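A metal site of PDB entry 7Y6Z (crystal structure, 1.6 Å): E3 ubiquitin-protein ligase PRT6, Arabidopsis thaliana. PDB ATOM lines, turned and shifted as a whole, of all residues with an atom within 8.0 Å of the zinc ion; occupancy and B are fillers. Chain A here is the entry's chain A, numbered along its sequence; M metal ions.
O of Cys 25 sits at hydrogen-bond distance from N of Lys 67 (2.9 Å). SG of Cys 22 lies close to N of Thr 24, at 3.6 Å.
The nearest printed residue that does not touch the zinc ion is Thr 24 (4.1 Å).
The zinc ion is bound by ND1 of His 46 (2.0 Å), ND1 of His 43 (2.1 Å), SG of Cys 22 (2.1 Å) and SG of Cys 25 (2.4 Å). The zinc ion has four donor atoms within binding distance.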
ATOM      1  N   ARG A  21       1.970 -20.182  12.606  1.00  0.00           N
ATOM      2  CA  ARG A  21       1.356 -21.360  12.046  1.00  0.00           C
ATOM      3  C   ARG A  21       2.413 -22.440  12.089  1.00  0.00           C
ATOM      4  O   ARG A  21       3.531 -22.231  11.646  1.00  0.00           O
ATOM      5  CB  ARG A  21       0.869 -21.093  10.600  1.00  0.00           C
ATOM      6  CG  ARG A  21       0.374 -22.427   9.986  1.00  0.00           C
ATOM      7  CD  ARG A  21      -0.458 -22.284   8.667  1.00  0.00           C
ATOM      8  NE  ARG A  21      -1.169 -23.579   8.348  1.00  0.00           N
ATOM      9  CZ  ARG A  21      -1.625 -23.850   7.128  1.00  0.00           C
ATOM     10  NH1 ARG A  21      -1.400 -22.982   6.137  1.00  0.00           N
ATOM     11  NH2 ARG A  21      -2.230 -24.996   6.886  1.00  0.00           N
ATOM     12  N   CYS A  22       2.039 -23.658  12.518  1.00  0.00           N
ATOM     13  CA  CYS A  22       2.944 -24.793  12.350  1.00  0.00           C
ATOM     14  C   CYS A  22       2.199 -25.937  11.679  1.00  0.00           C
ATOM     15  O   CYS A  22       1.340 -26.589  12.303  1.00  0.00           O
ATOM     16  CB  CYS A  22       3.558 -25.339  13.644  1.00  0.00           C
ATOM     17  SG  CYS A  22       4.745 -26.571  13.408  1.00  0.00           S
ATOM     18  N   ARG A  23       2.538 -26.148  10.446  1.00  0.00           N
ATOM     19  CA  ARG A  23       1.859 -27.192   9.659  1.00  0.00           C
ATOM     20  C   ARG A  23       2.171 -28.572  10.184  1.00  0.00           C
ATOM     21  O   ARG A  23       1.361 -29.499  10.014  1.00  0.00           O
ATOM     22  CB  ARG A  23       2.253 -27.019   8.201  1.00  0.00           C
ATOM     23  CG  ARG A  23       1.651 -25.824   7.548  1.00  0.00           C
ATOM     24  CD  ARG A  23       2.409 -25.409   6.316  1.00  0.00           C
ATOM     25  NE  ARG A  23       2.142 -24.043   5.873  1.00  0.00           N
ATOM     26  CZ  ARG A  23       2.711 -22.927   6.351  1.00  0.00           C
ATOM     27  NH1 ARG A  23       3.587 -22.926   7.358  1.00  0.00           N
ATOM     28  NH2 ARG A  23       2.357 -21.823   5.810  1.00  0.00           N
ATOM     29  N   THR A  24       3.301 -28.732  10.878  1.00  0.00           N
ATOM     30  CA  THR A  24       3.608 -30.018  11.477  1.00  0.00           C
ATOM     31  C   THR A  24       2.701 -30.309  12.668  1.00  0.00           C
ATOM     32  O   THR A  24       2.268 -31.436  12.855  1.00  0.00           O
ATOM     33  CB  THR A  24       5.069 -30.061  11.864  1.00  0.00           C
ATOM     34  OG1 THR A  24       5.846 -29.695  10.714  1.00  0.00           O
ATOM     35  CG2 THR A  24       5.524 -31.407  12.419  1.00  0.00           C
ATOM     36  N   CYS A  25       2.417 -29.320  13.489  1.00  0.00           N
ATOM     37  CA  CYS A  25       1.706 -29.511  14.763  1.00  0.00           C
ATOM     38  C   CYS A  25       0.207 -29.217  14.691  1.00  0.00           C
ATOM     39  O   CYS A  25      -0.570 -29.651  15.563  1.00  0.00           O
ATOM     40  CB  CYS A  25       2.332 -28.582  15.854  1.00  0.00           C
ATOM     41  SG  CYS A  25       3.952 -29.028  16.278  1.00  0.00           S
ATOM     42  N   GLU A  26      -0.242 -28.461  13.726  1.00  0.00           N
ATOM     43  CA  GLU A  26      -1.612 -27.996  13.783  1.00  0.00           C
ATOM     44  C   GLU A  26      -2.591 -29.156  13.675  1.00  0.00           C
ATOM     45  O   GLU A  26      -2.363 -30.116  12.916  1.00  0.00           O
ATOM     46  CB  GLU A  26      -1.916 -27.066  12.628  1.00  0.00           C
ATOM     47  CG  GLU A  26      -1.862 -27.688  11.237  1.00  0.00           C
ATOM     48  CD  GLU A  26      -1.831 -26.666  10.105  1.00  0.00           C
ATOM     49  OE1 GLU A  26      -1.499 -25.450  10.372  1.00  0.00           O
ATOM     50  OE2 GLU A  26      -2.121 -26.986   8.951  1.00  0.00           O
ATOM     51  N   ILE A  33      -0.464 -20.808  17.124  1.00  0.00           N
ATOM     52  CA  ILE A  33      -0.052 -20.591  18.512  1.00  0.00           C
ATOM     53  C   ILE A  33       0.647 -19.257  18.637  1.00  0.00           C
ATOM     54  O   ILE A  33       1.304 -18.801  17.687  1.00  0.00           O
ATOM     55  CB  ILE A  33       0.812 -21.692  19.118  1.00  0.00           C
ATOM     56  CG1 ILE A  33       2.080 -21.922  18.320  1.00  0.00           C
ATOM     57  CG2 ILE A  33      -0.065 -22.990  19.142  1.00  0.00           C
ATOM     58  CD1 ILE A  33       3.007 -22.886  19.033  1.00  0.00           C
ATOM     59  N   PHE A  38       5.168 -20.658  20.855  1.00  0.00           N
ATOM     60  CA  PHE A  38       6.067 -21.201  19.810  1.00  0.00           C
ATOM     61  C   PHE A  38       7.486 -21.250  20.289  1.00  0.00           C
ATOM     62  O   PHE A  38       8.227 -22.207  20.063  1.00  0.00           O
ATOM     63  CB  PHE A  38       6.018 -20.346  18.541  1.00  0.00           C
ATOM     64  CG  PHE A  38       6.923 -20.854  17.429  1.00  0.00           C
ATOM     65  CD1 PHE A  38       6.488 -21.895  16.589  1.00  0.00           C
ATOM     66  CD2 PHE A  38       8.196 -20.313  17.235  1.00  0.00           C
ATOM     67  CE1 PHE A  38       7.271 -22.349  15.548  1.00  0.00           C
ATOM     68  CE2 PHE A  38       8.999 -20.797  16.195  1.00  0.00           C
ATOM     69  CZ  PHE A  38       8.515 -21.821  15.366  1.00  0.00           C
ATOM     70  N   GLY A  41       8.431 -24.050  22.847  1.00  0.00           N
ATOM     71  CA  GLY A  41       8.278 -25.409  22.418  1.00  0.00           C
ATOM     72  C   GLY A  41       9.363 -25.778  21.442  1.00  0.00           C
ATOM     73  O   GLY A  41      10.315 -25.026  21.270  1.00  0.00           O
ATOM     74  N   ASP A  42       9.218 -26.942  20.781  1.00  0.00           N
ATOM     75  CA  ASP A  42      10.234 -27.464  19.872  1.00  0.00           C
ATOM     76  C   ASP A  42       9.617 -27.667  18.487  1.00  0.00           C
ATOM     77  O   ASP A  42       8.785 -28.579  18.293  1.00  0.00           O
ATOM     78  CB  ASP A  42      10.832 -28.735  20.430  1.00  0.00           C
ATOM     79  CG  ASP A  42      11.966 -29.295  19.575  1.00  0.00           C
ATOM     80  OD1 ASP A  42      12.258 -28.809  18.456  1.00  0.00           O
ATOM     81  OD2 ASP A  42      12.560 -30.282  20.057  1.00  0.00           O
ATOM     82  N   HIS A  43      10.021 -26.803  17.539  1.00  0.00           N
ATOM     83  CA  HIS A  43       9.535 -26.829  16.169  1.00  0.00           C
ATOM     84  C   HIS A  43      10.664 -26.826  15.129  1.00  0.00           C
ATOM     85  O   HIS A  43      10.457 -26.423  13.989  1.00  0.00           O
ATOM     86  CB  HIS A  43       8.572 -25.682  15.960  1.00  0.00           C
ATOM     87  CG  HIS A  43       7.430 -25.673  16.926  1.00  0.00           C
ATOM     88  ND1 HIS A  43       6.296 -26.403  16.702  1.00  0.00           N
ATOM     89  CD2 HIS A  43       7.250 -25.051  18.108  1.00  0.00           C
ATOM     90  CE1 HIS A  43       5.488 -26.281  17.745  1.00  0.00           C
ATOM     91  NE2 HIS A  43       6.006 -25.382  18.576  1.00  0.00           N
ATOM     92  N   ASN A  44      11.804 -27.438  15.474  1.00  0.00           N
ATOM     93  CA  ASN A  44      13.021 -27.283  14.674  1.00  0.00           C
ATOM     94  C   ASN A  44      12.860 -27.739  13.222  1.00  0.00           C
ATOM     95  O   ASN A  44      13.100 -26.966  12.284  1.00  0.00           O
ATOM     96  CB  ASN A  44      14.167 -28.041  15.354  1.00  0.00           C
ATOM     97  CG  ASN A  44      15.520 -27.647  14.807  1.00  0.00           C
ATOM     98  OD1 ASN A  44      15.709 -26.484  14.408  1.00  0.00           O
ATOM     99  ND2 ASN A  44      16.447 -28.579  14.766  1.00  0.00           N
ATOM    100  N   SER A  45      12.533 -29.001  13.002  1.00  0.00           N
ATOM    101  CA  SER A  45      12.420 -29.423  11.608  1.00  0.00           C
ATOM    102  C   SER A  45      11.098 -29.016  10.983  1.00  0.00           C
ATOM    103  O   SER A  45      10.810 -29.404   9.831  1.00  0.00           O
ATOM    104  CB  SER A  45      12.581 -30.946  11.536  1.00  0.00           C
ATOM    105  OG  SER A  45      11.857 -31.587  12.590  1.00  0.00           O
ATOM    106  N   HIS A  46      10.241 -28.323  11.737  1.00  0.00           N
ATOM    107  CA  HIS A  46       8.830 -28.185  11.427  1.00  0.00           C
ATOM    108  C   HIS A  46       8.605 -27.148  10.337  1.00  0.00           C
ATOM    109  O   HIS A  46       9.449 -26.293  10.100  1.00  0.00           O
ATOM    110  CB  HIS A  46       8.055 -27.773  12.683  1.00  0.00           C
ATOM    111  CG  HIS A  46       7.949 -28.853  13.716  1.00  0.00           C
ATOM    112  ND1 HIS A  46       6.868 -28.960  14.556  1.00  0.00           N
ATOM    113  CD2 HIS A  46       8.810 -29.841  14.077  1.00  0.00           C
ATOM    114  CE1 HIS A  46       7.032 -30.006  15.360  1.00  0.00           C
ATOM    115  NE2 HIS A  46       8.221 -30.532  15.116  1.00  0.00           N
ATOM    116  N   ASP A  47       7.435 -27.228   9.704  1.00  0.00           N
ATOM    117  CA  ASP A  47       7.061 -26.353   8.618  1.00  0.00           C
ATOM    118  C   ASP A  47       6.164 -25.257   9.178  1.00  0.00           C
ATOM    119  O   ASP A  47       4.942 -25.261   9.062  1.00  0.00           O
ATOM    120  CB  ASP A  47       6.418 -27.094   7.465  1.00  0.00           C
ATOM    121  CG  ASP A  47       6.173 -26.162   6.294  1.00  0.00           C
ATOM    122  OD1 ASP A  47       6.633 -24.994   6.358  1.00  0.00           O
ATOM    123  OD2 ASP A  47       5.545 -26.597   5.311  1.00  0.00           O
ATOM    124  N   TYR A  48       6.835 -24.287   9.776  1.00  0.00           N
ATOM    125  CA  TYR A  48       6.154 -23.213  10.490  1.00  0.00           C
ATOM    126  C   TYR A  48       6.344 -21.908   9.715  1.00  0.00           C
ATOM    127  O   TYR A  48       7.241 -21.769   8.865  1.00  0.00           O
ATOM    128  CB  TYR A  48       6.687 -23.078  11.928  1.00  0.00           C
ATOM    129  CG  TYR A  48       8.143 -22.777  12.028  1.00  0.00           C
ATOM    130  CD1 TYR A  48       8.616 -21.484  11.956  1.00  0.00           C
ATOM    131  CD2 TYR A  48       9.033 -23.779  12.258  1.00  0.00           C
ATOM    132  CE1 TYR A  48       9.958 -21.223  12.042  1.00  0.00           C
ATOM    133  CE2 TYR A  48      10.341 -23.556  12.373  1.00  0.00           C
ATOM    134  CZ  TYR A  48      10.817 -22.261  12.291  1.00  0.00           C
ATOM    135  OH  TYR A  48      12.159 -22.031  12.416  1.00  0.00           O
ATOM    136  N   TRP A  66      -4.265 -28.820  18.584  1.00  0.00           N
ATOM    137  CA  TRP A  66      -2.825 -28.824  18.410  1.00  0.00           C
ATOM    138  C   TRP A  66      -2.292 -30.136  18.926  1.00  0.00           C
ATOM    139  O   TRP A  66      -2.730 -30.634  19.966  1.00  0.00           O
ATOM    140  CB  TRP A  66      -2.255 -27.633  19.179  1.00  0.00           C
ATOM    141  CG  TRP A  66      -0.902 -27.145  18.790  1.00  0.00           C
ATOM    142  CD1 TRP A  66       0.267 -27.417  19.427  1.00  0.00           C
ATOM    143  CD2 TRP A  66      -0.566 -26.258  17.673  1.00  0.00           C
ATOM    144  NE1 TRP A  66       1.308 -26.796  18.771  1.00  0.00           N
ATOM    145  CE2 TRP A  66       0.823 -26.059  17.711  1.00  0.00           C
ATOM    146  CE3 TRP A  66      -1.317 -25.603  16.713  1.00  0.00           C
ATOM    147  CZ2 TRP A  66       1.481 -25.192  16.838  1.00  0.00           C
ATOM    148  CZ3 TRP A  66      -0.712 -24.825  15.794  1.00  0.00           C
ATOM    149  CH2 TRP A  66       0.709 -24.622  15.851  1.00  0.00           C
ATOM    150  N   LYS A  67      -1.301 -30.660  18.207  1.00  0.00           N
ATOM    151  CA  LYS A  67      -0.703 -31.925  18.600  1.00  0.00           C
ATOM    152  C   LYS A  67       0.117 -31.758  19.885  1.00  0.00           C
ATOM    153  O   LYS A  67       0.864 -30.780  20.036  1.00  0.00           O
ATOM    154  CB  LYS A  67       0.168 -32.477  17.453  1.00  0.00           C
ATOM    155  CG  LYS A  67      -0.620 -32.853  16.158  1.00  0.00           C
ATOM    156  CD  LYS A  67       0.325 -33.285  15.076  1.00  0.00           C
ATOM    157  CE  LYS A  67      -0.385 -33.191  13.760  1.00  0.00           C
ATOM    158  NZ  LYS A  67       0.412 -33.680  12.561  1.00  0.00           N
ATOM    159  N   ASP A  69       2.755 -32.928  21.159  1.00  0.00           N
ATOM    160  CA  ASP A  69       4.188 -32.814  21.062  1.00  0.00           C
ATOM    161  C   ASP A  69       4.593 -31.386  20.669  1.00  0.00           C
ATOM    162  O   ASP A  69       5.766 -31.035  20.799  1.00  0.00           O
ATOM    163  CB  ASP A  69       4.837 -33.800  20.071  1.00  0.00           C
ATOM    164  CG  ASP A  69       4.288 -33.697  18.630  1.00  0.00           C
ATOM    165  OD1 ASP A  69       5.027 -33.253  17.688  1.00  0.00           O
ATOM    166  OD2 ASP A  69       3.121 -34.066  18.426  1.00  0.00           O
ATOM    167  N   GLY A  70       3.656 -30.593  20.139  1.00  0.00           N
ATOM    168  CA  GLY A  70       3.872 -29.185  19.873  1.00  0.00           C
ATOM    169  C   GLY A  70       3.495 -28.221  20.959  1.00  0.00           C
ATOM    170  O   GLY A  70       3.684 -26.995  20.766  1.00  0.00           O
ATOM    171  N   PHE A  71       3.064 -28.705  22.117  1.00  0.00           N
ATOM    172  CA  PHE A  71       2.808 -27.861  23.279  1.00  0.00           C
ATOM    173  C   PHE A  71       4.121 -27.273  23.808  1.00  0.00           C
ATOM    174  O   PHE A  71       5.203 -27.870  23.673  1.00  0.00           O
ATOM    175  CB  PHE A  71       2.165 -28.661  24.404  1.00  0.00           C
ATOM    176  CG  PHE A  71       0.785 -29.176  24.107  1.00  0.00           C
ATOM    177  CD1 PHE A  71       0.155 -30.039  24.957  1.00  0.00           C
ATOM    178  CD2 PHE A  71       0.109 -28.760  22.957  1.00  0.00           C
ATOM    179  CE1 PHE A  71      -1.127 -30.513  24.649  1.00  0.00           C
ATOM    180  CE2 PHE A  71      -1.151 -29.105  22.713  1.00  0.00           C
ATOM    181  CZ  PHE A  71      -1.795 -30.004  23.555  1.00  0.00           C
HETATM  182 ZN    ZN M   1       5.509 -27.566  15.146  1.00  0.00          ZN
